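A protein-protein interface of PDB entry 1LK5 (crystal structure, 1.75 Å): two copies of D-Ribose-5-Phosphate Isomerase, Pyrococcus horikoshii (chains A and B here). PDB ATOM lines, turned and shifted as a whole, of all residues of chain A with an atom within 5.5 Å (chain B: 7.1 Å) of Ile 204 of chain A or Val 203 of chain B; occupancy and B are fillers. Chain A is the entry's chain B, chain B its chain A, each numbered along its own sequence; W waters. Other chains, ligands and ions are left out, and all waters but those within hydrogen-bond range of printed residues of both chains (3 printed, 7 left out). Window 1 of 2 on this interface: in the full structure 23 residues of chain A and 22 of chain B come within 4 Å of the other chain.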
ATOM      1  N   THR A 105      -7.668  -2.649  38.811  1.00  0.00           N
ATOM      2  CA  THR A 105      -7.788  -1.827  37.626  1.00  0.00           C
ATOM      3  C   THR A 105      -8.737  -0.646  37.821  1.00  0.00           C
ATOM      4  O   THR A 105      -8.358   0.502  37.586  1.00  0.00           O
ATOM      5  CB  THR A 105      -8.211  -2.688  36.425  1.00  0.00           C
ATOM      6  OG1 THR A 105      -7.113  -3.537  36.067  1.00  0.00           O
ATOM      7  CG2 THR A 105      -8.431  -1.839  35.190  1.00  0.00           C
ATOM      8  N   GLU A 139      -2.996  -7.924  36.745  1.00  0.00           N
ATOM      9  CA  GLU A 139      -4.121  -8.295  35.891  1.00  0.00           C
ATOM     10  C   GLU A 139      -3.659  -8.434  34.438  1.00  0.00           C
ATOM     11  O   GLU A 139      -3.039  -7.530  33.884  1.00  0.00           O
ATOM     12  CB  GLU A 139      -5.266  -7.295  35.989  1.00  0.00           C
ATOM     13  CG  GLU A 139      -6.481  -7.700  35.166  1.00  0.00           C
ATOM     14  CD  GLU A 139      -7.747  -6.945  35.557  1.00  0.00           C
ATOM     15  OE1 GLU A 139      -7.691  -6.169  36.523  1.00  0.00           O
ATOM     16  OE2 GLU A 139      -8.791  -7.124  34.892  1.00  0.00           O
ATOM     17  N   VAL A 140      -3.959  -9.578  33.849  1.00  0.00           N
ATOM     18  CA  VAL A 140      -3.479  -9.892  32.503  1.00  0.00           C
ATOM     19  C   VAL A 140      -4.555 -10.431  31.576  1.00  0.00           C
ATOM     20  O   VAL A 140      -5.465 -11.151  32.000  1.00  0.00           O
ATOM     21  CB  VAL A 140      -2.317 -10.926  32.561  1.00  0.00           C
ATOM     22  CG1 VAL A 140      -1.207 -10.413  33.470  1.00  0.00           C
ATOM     23  CG2 VAL A 140      -2.811 -12.303  33.053  1.00  0.00           C
ATOM     24  N   ILE A 141      -4.410 -10.093  30.297  1.00  0.00           N
ATOM     25  CA  ILE A 141      -5.222 -10.667  29.236  1.00  0.00           C
ATOM     26  C   ILE A 141      -4.949 -12.166  29.315  1.00  0.00           C
ATOM     27  O   ILE A 141      -3.778 -12.588  29.320  1.00  0.00           O
ATOM     28  CB  ILE A 141      -4.797 -10.126  27.848  1.00  0.00           C
ATOM     29  CG1 ILE A 141      -4.997  -8.607  27.731  1.00  0.00           C
ATOM     30  CG2 ILE A 141      -5.524 -10.880  26.763  1.00  0.00           C
ATOM     31  CD1 ILE A 141      -6.432  -8.133  27.877  1.00  0.00           C
ATOM     32  N   ASN A 175     -13.251  -7.506  34.699  1.00  0.00           N
ATOM     33  CA  ASN A 175     -12.997  -7.177  33.292  1.00  0.00           C
ATOM     34  C   ASN A 175     -12.736  -8.404  32.409  1.00  0.00           C
ATOM     35  O   ASN A 175     -12.366  -8.253  31.235  1.00  0.00           O
ATOM     36  CB  ASN A 175     -11.812  -6.218  33.201  1.00  0.00           C
ATOM     37  CG  ASN A 175     -11.798  -5.222  34.332  1.00  0.00           C
ATOM     38  OD1 ASN A 175     -11.065  -5.396  35.351  1.00  0.00           O
ATOM     39  ND2 ASN A 175     -12.650  -4.212  34.216  1.00  0.00           N
ATOM     40  N   ASN A 177     -10.465 -10.773  32.907  1.00  0.00           N
ATOM     41  CA  ASN A 177      -9.052 -11.147  32.877  1.00  0.00           C
ATOM     42  C   ASN A 177      -8.593 -12.072  34.007  1.00  0.00           C
ATOM     43  O   ASN A 177      -9.332 -12.364  34.943  1.00  0.00           O
ATOM     44  CB  ASN A 177      -8.212  -9.877  32.865  1.00  0.00           C
ATOM     45  CG  ASN A 177      -8.539  -8.996  31.678  1.00  0.00           C
ATOM     46  OD1 ASN A 177      -8.632  -9.482  30.549  1.00  0.00           O
ATOM     47  ND2 ASN A 177      -8.719  -7.701  31.923  1.00  0.00           N
ATOM     48  N   ASN A 198       3.528  -2.425  33.790  1.00  0.00           N
ATOM     49  CA  ASN A 198       2.495  -1.957  32.867  1.00  0.00           C
ATOM     50  C   ASN A 198       2.981  -1.877  31.412  1.00  0.00           C
ATOM     51  O   ASN A 198       2.179  -1.977  30.496  1.00  0.00           O
ATOM     52  CB  ASN A 198       1.851  -0.647  33.341  1.00  0.00           C
ATOM     53  CG  ASN A 198       0.844  -0.879  34.443  1.00  0.00           C
ATOM     54  OD1 ASN A 198       0.340  -1.984  34.601  1.00  0.00           O
ATOM     55  ND2 ASN A 198       0.567   0.151  35.239  1.00  0.00           N
ATOM     56  N   GLY A 202       0.130  -7.292  27.478  1.00  0.00           N
ATOM     57  CA  GLY A 202      -0.703  -8.279  28.132  1.00  0.00           C
ATOM     58  C   GLY A 202      -0.982  -7.899  29.571  1.00  0.00           C
ATOM     59  O   GLY A 202      -1.959  -8.369  30.157  1.00  0.00           O
ATOM     60  N   VAL A 203      -0.120  -7.081  30.169  1.00  0.00           N
ATOM     61  CA  VAL A 203      -0.401  -6.596  31.513  1.00  0.00           C
ATOM     62  C   VAL A 203      -1.298  -5.389  31.379  1.00  0.00           C
ATOM     63  O   VAL A 203      -0.923  -4.421  30.722  1.00  0.00           O
ATOM     64  CB  VAL A 203       0.868  -6.186  32.264  1.00  0.00           C
ATOM     65  CG1 VAL A 203       0.514  -5.489  33.594  1.00  0.00           C
ATOM     66  CG2 VAL A 203       1.727  -7.400  32.516  1.00  0.00           C
ATOM     67  N   ILE A 204      -2.464  -5.398  32.011  1.00  0.00           N
ATOM     68  CA  ILE A 204      -3.289  -4.197  31.900  1.00  0.00           C
ATOM     69  C   ILE A 204      -3.238  -3.311  33.135  1.00  0.00           C
ATOM     70  O   ILE A 204      -3.540  -2.125  33.046  1.00  0.00           O
ATOM     71  CB  ILE A 204      -4.720  -4.484  31.471  1.00  0.00           C
ATOM     72  CG1 ILE A 204      -5.522  -5.126  32.596  1.00  0.00           C
ATOM     73  CG2 ILE A 204      -4.744  -5.329  30.222  1.00  0.00           C
ATOM     74  CD1 ILE A 204      -6.976  -4.803  32.473  1.00  0.00           C
ATOM     75  N   GLU A 205      -2.878  -3.893  34.272  1.00  0.00           N
ATOM     76  CA  GLU A 205      -2.646  -3.113  35.489  1.00  0.00           C
ATOM     77  C   GLU A 205      -1.916  -3.980  36.512  1.00  0.00           C
ATOM     78  O   GLU A 205      -1.954  -5.201  36.426  1.00  0.00           O
ATOM     79  CB  GLU A 205      -3.968  -2.639  36.070  1.00  0.00           C
ATOM     80  CG  GLU A 205      -3.795  -1.664  37.216  1.00  0.00           C
ATOM     81  CD  GLU A 205      -2.923  -0.497  36.825  1.00  0.00           C
ATOM     82  OE1 GLU A 205      -1.712  -0.534  37.135  1.00  0.00           O
ATOM     83  OE2 GLU A 205      -3.425   0.459  36.195  1.00  0.00           O
ATOM     84  N   ASN A 206      -1.228  -3.351  37.457  1.00  0.00           N
ATOM     85  CA  ASN A 206      -0.577  -4.078  38.539  1.00  0.00           C
ATOM     86  C   ASN A 206      -0.832  -3.414  39.876  1.00  0.00           C
ATOM     87  O   ASN A 206      -1.135  -2.218  39.945  1.00  0.00           O
ATOM     88  CB  ASN A 206       0.925  -4.268  38.296  1.00  0.00           C
ATOM     89  CG  ASN A 206       1.700  -2.973  38.353  1.00  0.00           C
ATOM     90  OD1 ASN A 206       2.171  -2.581  39.417  1.00  0.00           O
ATOM     91  ND2 ASN A 206       1.834  -2.301  37.214  1.00  0.00           N
ATOM     92  N   THR B 105      -4.110  -5.072  20.833  1.00  0.00           N
ATOM     93  CA  THR B 105      -3.686  -5.694  22.082  1.00  0.00           C
ATOM     94  C   THR B 105      -3.126  -7.095  21.867  1.00  0.00           C
ATOM     95  O   THR B 105      -2.001  -7.393  22.297  1.00  0.00           O
ATOM     96  CB  THR B 105      -4.850  -5.684  23.088  1.00  0.00           C
ATOM     97  OG1 THR B 105      -5.115  -4.323  23.463  1.00  0.00           O
ATOM     98  CG2 THR B 105      -4.471  -6.349  24.375  1.00  0.00           C
ATOM     99  N   ILE B 138      -5.939   3.658  20.838  1.00  0.00           N
ATOM    100  CA  ILE B 138      -5.634   3.334  22.218  1.00  0.00           C
ATOM    101  C   ILE B 138      -6.829   2.562  22.763  1.00  0.00           C
ATOM    102  O   ILE B 138      -7.943   3.071  22.743  1.00  0.00           O
ATOM    103  CB  ILE B 138      -5.418   4.607  23.071  1.00  0.00           C
ATOM    104  CG1 ILE B 138      -4.279   5.453  22.498  1.00  0.00           C
ATOM    105  CG2 ILE B 138      -5.120   4.215  24.516  1.00  0.00           C
ATOM    106  CD1 ILE B 138      -4.125   6.810  23.184  1.00  0.00           C
ATOM    107  N   GLU B 139      -6.594   1.351  23.253  1.00  0.00           N
ATOM    108  CA  GLU B 139      -7.653   0.527  23.809  1.00  0.00           C
ATOM    109  C   GLU B 139      -7.750   0.847  25.285  1.00  0.00           C
ATOM    110  O   GLU B 139      -6.740   0.863  25.978  1.00  0.00           O
ATOM    111  CB  GLU B 139      -7.367  -0.969  23.621  1.00  0.00           C
ATOM    112  CG  GLU B 139      -8.468  -1.869  24.164  1.00  0.00           C
ATOM    113  CD  GLU B 139      -8.408  -3.295  23.637  1.00  0.00           C
ATOM    114  OE1 GLU B 139      -7.599  -3.575  22.732  1.00  0.00           O
ATOM    115  OE2 GLU B 139      -9.172  -4.131  24.135  1.00  0.00           O
ATOM    116  N   VAL B 140      -8.967   1.083  25.753  1.00  0.00           N
ATOM    117  CA  VAL B 140      -9.178   1.534  27.115  1.00  0.00           C
ATOM    118  C   VAL B 140     -10.369   0.880  27.780  1.00  0.00           C
ATOM    119  O   VAL B 140     -11.341   0.507  27.136  1.00  0.00           O
ATOM    120  CB  VAL B 140      -9.387   3.084  27.185  1.00  0.00           C
ATOM    121  CG1 VAL B 140      -8.219   3.829  26.523  1.00  0.00           C
ATOM    122  CG2 VAL B 140     -10.695   3.511  26.568  1.00  0.00           C
ATOM    123  N   ILE B 141     -10.272   0.749  29.093  1.00  0.00           N
ATOM    124  CA  ILE B 141     -11.392   0.305  29.899  1.00  0.00           C
ATOM    125  C   ILE B 141     -12.509   1.327  29.658  1.00  0.00           C
ATOM    126  O   ILE B 141     -12.291   2.528  29.786  1.00  0.00           O
ATOM    127  CB  ILE B 141     -10.992   0.270  31.385  1.00  0.00           C
ATOM    128  CG1 ILE B 141      -9.920  -0.810  31.626  1.00  0.00           C
ATOM    129  CG2 ILE B 141     -12.222   0.083  32.244  1.00  0.00           C
ATOM    130  CD1 ILE B 141     -10.440  -2.236  31.673  1.00  0.00           C
ATOM    131  N   ALA B 144     -13.084   4.731  31.558  1.00  0.00           N
ATOM    132  CA  ALA B 144     -11.974   5.668  31.566  1.00  0.00           C
ATOM    133  C   ALA B 144     -11.892   6.499  30.287  1.00  0.00           C
ATOM    134  O   ALA B 144     -11.047   7.377  30.180  1.00  0.00           O
ATOM    135  CB  ALA B 144     -10.665   4.911  31.769  1.00  0.00           C
ATOM    136  N   ILE B 148      -9.381   9.914  29.786  1.00  0.00           N
ATOM    137  CA  ILE B 148      -8.172   9.707  29.007  1.00  0.00           C
ATOM    138  C   ILE B 148      -8.094  10.690  27.847  1.00  0.00           C
ATOM    139  O   ILE B 148      -7.023  11.259  27.590  1.00  0.00           O
ATOM    140  CB  ILE B 148      -8.047   8.252  28.547  1.00  0.00           C
ATOM    141  CG1 ILE B 148      -7.702   7.381  29.751  1.00  0.00           C
ATOM    142  CG2 ILE B 148      -6.966   8.147  27.480  1.00  0.00           C
ATOM    143  CD1 ILE B 148      -7.856   5.904  29.550  1.00  0.00           C
ATOM    144  N   LEU B 152      -5.093  13.587  27.414  1.00  0.00           N
ATOM    145  CA  LEU B 152      -4.200  13.596  26.265  1.00  0.00           C
ATOM    146  C   LEU B 152      -4.101  14.982  25.606  1.00  0.00           C
ATOM    147  O   LEU B 152      -3.241  15.211  24.749  1.00  0.00           O
ATOM    148  CB  LEU B 152      -4.612  12.524  25.259  1.00  0.00           C
ATOM    149  CG  LEU B 152      -4.378  11.085  25.744  1.00  0.00           C
ATOM    150  CD1 LEU B 152      -4.923  10.101  24.741  1.00  0.00           C
ATOM    151  CD2 LEU B 152      -2.915  10.822  25.983  1.00  0.00           C
ATOM    152  N   ASN B 177     -13.446  -3.781  25.246  1.00  0.00           N
ATOM    153  CA  ASN B 177     -13.063  -2.417  25.573  1.00  0.00           C
ATOM    154  C   ASN B 177     -13.383  -1.424  24.483  1.00  0.00           C
ATOM    155  O   ASN B 177     -13.831  -1.805  23.399  1.00  0.00           O
ATOM    156  CB  ASN B 177     -11.562  -2.383  25.897  1.00  0.00           C
ATOM    157  CG  ASN B 177     -11.225  -3.245  27.066  1.00  0.00           C
ATOM    158  OD1 ASN B 177     -11.890  -3.177  28.104  1.00  0.00           O
ATOM    159  ND2 ASN B 177     -10.223  -4.128  26.896  1.00  0.00           N
ATOM    160  N   GLU B 194       4.990   5.647  23.894  1.00  0.00           N
ATOM    161  CA  GLU B 194       4.373   4.324  24.063  1.00  0.00           C
ATOM    162  C   GLU B 194       4.323   3.952  25.553  1.00  0.00           C
ATOM    163  O   GLU B 194       3.317   3.423  26.046  1.00  0.00           O
ATOM    164  CB  GLU B 194       5.161   3.290  23.254  1.00  0.00           C
ATOM    165  CG  GLU B 194       4.508   1.912  23.205  1.00  0.00           C
ATOM    166  CD  GLU B 194       5.307   0.894  22.402  1.00  0.00           C
ATOM    167  OE1 GLU B 194       5.032  -0.325  22.561  1.00  0.00           O
ATOM    168  OE2 GLU B 194       6.172   1.302  21.583  1.00  0.00           O
ATOM    169  N   GLU B 196       4.568   6.201  28.123  1.00  0.00           N
ATOM    170  CA  GLU B 196       3.682   7.169  28.742  1.00  0.00           C
ATOM    171  C   GLU B 196       2.217   6.738  28.642  1.00  0.00           C
ATOM    172  O   GLU B 196       1.491   6.777  29.629  1.00  0.00           O
ATOM    173  CB  GLU B 196       3.897   8.546  28.105  1.00  0.00           C
ATOM    174  CG  GLU B 196       2.723   9.504  28.152  1.00  0.00           C
ATOM    175  CD  GLU B 196       2.267   9.834  29.546  1.00  0.00           C
ATOM    176  OE1 GLU B 196       1.147  10.373  29.676  1.00  0.00           O
ATOM    177  OE2 GLU B 196       3.012   9.545  30.499  1.00  0.00           O
ATOM    178  N   LEU B 197       1.796   6.295  27.467  1.00  0.00           N
ATOM    179  CA  LEU B 197       0.386   5.941  27.279  1.00  0.00           C
ATOM    180  C   LEU B 197       0.054   4.704  28.101  1.00  0.00           C
ATOM    181  O   LEU B 197      -1.014   4.633  28.704  1.00  0.00           O
ATOM    182  CB  LEU B 197       0.044   5.743  25.805  1.00  0.00           C
ATOM    183  CG  LEU B 197       0.132   6.978  24.903  1.00  0.00           C
ATOM    184  CD1 LEU B 197      -0.113   6.573  23.502  1.00  0.00           C
ATOM    185  CD2 LEU B 197      -0.852   8.071  25.337  1.00  0.00           C
ATOM    186  N   ASN B 198       0.993   3.766  28.180  1.00  0.00           N
ATOM    187  CA  ASN B 198       0.770   2.572  28.981  1.00  0.00           C
ATOM    188  C   ASN B 198       0.792   2.802  30.492  1.00  0.00           C
ATOM    189  O   ASN B 198       0.338   1.940  31.244  1.00  0.00           O
ATOM    190  CB  ASN B 198       1.713   1.431  28.554  1.00  0.00           C
ATOM    191  CG  ASN B 198       1.190   0.691  27.325  1.00  0.00           C
ATOM    192  OD1 ASN B 198      -0.010   0.692  27.060  1.00  0.00           O
ATOM    193  ND2 ASN B 198       2.092   0.088  26.546  1.00  0.00           N
ATOM    194  N   THR B 199       1.308   3.949  30.932  1.00  0.00           N
ATOM    195  CA  THR B 199       1.302   4.299  32.358  1.00  0.00           C
ATOM    196  C   THR B 199       0.022   4.995  32.774  1.00  0.00           C
ATOM    197  O   THR B 199      -0.150   5.289  33.964  1.00  0.00           O
ATOM    198  CB  THR B 199       2.485   5.232  32.769  1.00  0.00           C
ATOM    199  OG1 THR B 199       2.311   6.545  32.217  1.00  0.00           O
ATOM    200  CG2 THR B 199       3.804   4.750  32.246  1.00  0.00           C
ATOM    201  N   ILE B 200      -0.877   5.269  31.836  1.00  0.00           N
ATOM    202  CA  ILE B 200      -2.134   5.946  32.187  1.00  0.00           C
ATOM    203  C   ILE B 200      -3.139   4.909  32.647  1.00  0.00           C
ATOM    204  O   ILE B 200      -3.471   4.028  31.874  1.00  0.00           O
ATOM    205  CB  ILE B 200      -2.720   6.690  30.976  1.00  0.00           C
ATOM    206  CG1 ILE B 200      -1.806   7.833  30.537  1.00  0.00           C
ATOM    207  CG2 ILE B 200      -4.144   7.176  31.312  1.00  0.00           C
ATOM    208  CD1 ILE B 200      -2.196   8.442  29.217  1.00  0.00           C
ATOM    209  N   PRO B 201      -3.605   4.968  33.898  1.00  0.00           N
ATOM    210  CA  PRO B 201      -4.598   3.998  34.357  1.00  0.00           C
ATOM    211  C   PRO B 201      -5.834   4.002  33.467  1.00  0.00           C
ATOM    212  O   PRO B 201      -6.438   5.046  33.207  1.00  0.00           O
ATOM    213  CB  PRO B 201      -4.904   4.458  35.790  1.00  0.00           C
ATOM    214  CG  PRO B 201      -3.638   5.125  36.204  1.00  0.00           C
ATOM    215  CD  PRO B 201      -3.179   5.865  34.986  1.00  0.00           C
ATOM    216  N   GLY B 202      -6.181   2.824  32.975  1.00  0.00           N
ATOM    217  CA  GLY B 202      -7.301   2.688  32.071  1.00  0.00           C
ATOM    218  C   GLY B 202      -6.870   2.253  30.692  1.00  0.00           C
ATOM    219  O   GLY B 202      -7.670   1.698  29.955  1.00  0.00           O
ATOM    220  N   VAL B 203      -5.618   2.512  30.337  1.00  0.00           N
ATOM    221  CA  VAL B 203      -5.102   2.080  29.038  1.00  0.00           C
ATOM    222  C   VAL B 203      -4.721   0.590  29.105  1.00  0.00           C
ATOM    223  O   VAL B 203      -3.960   0.158  29.981  1.00  0.00           O
ATOM    224  CB  VAL B 203      -3.910   2.956  28.562  1.00  0.00           C
ATOM    225  CG1 VAL B 203      -3.264   2.379  27.297  1.00  0.00           C
ATOM    226  CG2 VAL B 203      -4.344   4.384  28.312  1.00  0.00           C
ATOM    227  N   ILE B 204      -5.298  -0.185  28.186  1.00  0.00           N
ATOM    228  CA  ILE B 204      -5.060  -1.611  28.037  1.00  0.00           C
ATOM    229  C   ILE B 204      -3.784  -1.804  27.212  1.00  0.00           C
ATOM    230  O   ILE B 204      -2.902  -2.603  27.554  1.00  0.00           O
ATOM    231  CB  ILE B 204      -6.277  -2.227  27.276  1.00  0.00           C
ATOM    232  CG1 ILE B 204      -7.589  -2.035  28.068  1.00  0.00           C
ATOM    233  CG2 ILE B 204      -6.060  -3.682  26.948  1.00  0.00           C
ATOM    234  CD1 ILE B 204      -7.686  -2.837  29.334  1.00  0.00           C
ATOM    235  N   GLU B 205      -3.724  -1.058  26.123  1.00  0.00           N
ATOM    236  CA  GLU B 205      -2.600  -1.070  25.202  1.00  0.00           C
ATOM    237  C   GLU B 205      -2.748   0.091  24.242  1.00  0.00           C
ATOM    238  O   GLU B 205      -3.840   0.621  24.047  1.00  0.00           O
ATOM    239  CB  GLU B 205      -2.552  -2.386  24.424  1.00  0.00           C
ATOM    240  CG  GLU B 205      -1.306  -2.576  23.563  1.00  0.00           C
ATOM    241  CD  GLU B 205      -0.038  -2.401  24.351  1.00  0.00           C
ATOM    242  OE1 GLU B 205       0.583  -1.305  24.263  1.00  0.00           O
ATOM    243  OE2 GLU B 205       0.317  -3.350  25.084  1.00  0.00           O
ATOM    244  N   ASN B 206      -1.649   0.501  23.624  1.00  0.00           N
ATOM    245  CA  ASN B 206      -1.707   1.595  22.664  1.00  0.00           C
ATOM    246  C   ASN B 206      -1.050   1.174  21.347  1.00  0.00           C
ATOM    247  O   ASN B 206      -0.235   0.261  21.318  1.00  0.00           O
ATOM    248  CB  ASN B 206      -1.076   2.872  23.230  1.00  0.00           C
ATOM    249  CG  ASN B 206       0.411   2.771  23.375  1.00  0.00           C
ATOM    250  OD1 ASN B 206       1.145   3.069  22.435  1.00  0.00           O
ATOM    251  ND2 ASN B 206       0.882   2.363  24.567  1.00  0.00           N
HETATM  252  O   HOH W   1      -9.596  -5.993  29.395  1.00  0.00           O
HETATM  253  O   HOH W   2      -6.113   0.931  35.738  1.00  0.00           O
HETATM  254  O   HOH W   3     -12.334  -5.303  29.797  1.00  0.00           O
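Hydrophobic or aromatic side chains of chain B that line the printed part of chain A: Ile 141 and Ile 204. Along chain B the printed residues that touch a printed residue of chain A span positions 141 to 204. Hydrophobic or aromatic side chains of chain A within 4 Å of the printed part of chain B: Ile 204. Among the printed residues, 5 pairs touch across the chains. Among the printed residues, no Asp or Glu carboxylate lies within 4 Å of a Lys or Arg side-chain nitrogen of the other chain.
Among the printed residues, merely in contact across the chains: Asn 198 of chain A with Asn 198 of chain B, Ile 204 of chain A with Ile 204 of chain B, Ile 204 of chain A with Val 203 of chain B, Asn 175 of chain A with Ile 141 of chain B and Thr 105 of chain A with Ile 141 of chain B.
Printed residues of chain B within 4 Å of Asn 175 of chain A: Ile 141 (3.9 Å). Of the printed residues of chain B, Asn 198 of chain A touches Asn 198 (3.7 Å). Of chain B, only Val 203 and Ile 204 come within 4 Å of Ile 204 of chain A. Of the printed residues of chain A, Ile 141 of chain B touches Thr 105 and Asn 175. Glu 194 of chain B touches none of the printed residues of chain A. Of the printed residues of chain A, Asn 198 of chain B touches Asn 198. Pro 201 of chain B touches none of the printed residues of chain A. Of the printed residues of chain A, Ile 204 of chain B touches Ile 204 (3.8 Å). The nearest residue of chain B that does not touch Ile 204 of chain A is Ile 141 of chain B (4.4 Å).
Thr 105 of chain A touches Ile 141 of chain B, but with the chains exchanged Ile 141 of chain A does not touch Thr 105 of chain B (4.1 Å). Asn 198 of chain A touches its own counterpart, Asn 198 of chain B. Ile 204 of chain A touches Val 203 of chain B, but with the chains exchanged Val 203 of chain A does not touch Ile 204 of chain B (4.2 Å). Ile 204 of chain A touches its own counterpart, Ile 204 of chain B. 11 positions are printed for both chains.
Water W3 lies within hydrogen-bond range of OD1 of Asn 177 of chain B (2.8 Å) and O of Asn 175 of chain A (3.3 Å). Water W2 lies within hydrogen-bond range of OE2 of Glu 205 of chain A (2.8 Å), O of Thr 105 of chain A (2.9 Å) and N of Gly 202 of chain B (3.3 Å). Water W1 lies within hydrogen-bond range of ND2 of Asn 177 of chain A (3.2 Å) and ND2 of Asn 177 of chain B (3.2 Å).
OD1 of Asn 198 of chain B is in hydrogen-bond range of ND2 of Asn 206 of chain B (3.1 Å). The side-chain amide nitrogen of Asn 198 of chain B sits at hydrogen-bond distance from the side-chain carboxylate of Glu 205 of chain B (3.1 Å). ND2 of Asn 206 of chain A is in hydrogen-bond range of OD1 of Asn 198 of chain A. The backbone carbonyl oxygen of Glu 139 of chain B sits at hydrogen-bond distance from the backbone NH of Ile 204 of chain B. O of Glu 139 of chain A lies within hydrogen-bond range of N of Ile 204 of chain A (2.9 Å). OE2 of Glu 139 of chain A lies close to OD1 of Asn 175 of chain A (2.9 Å).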
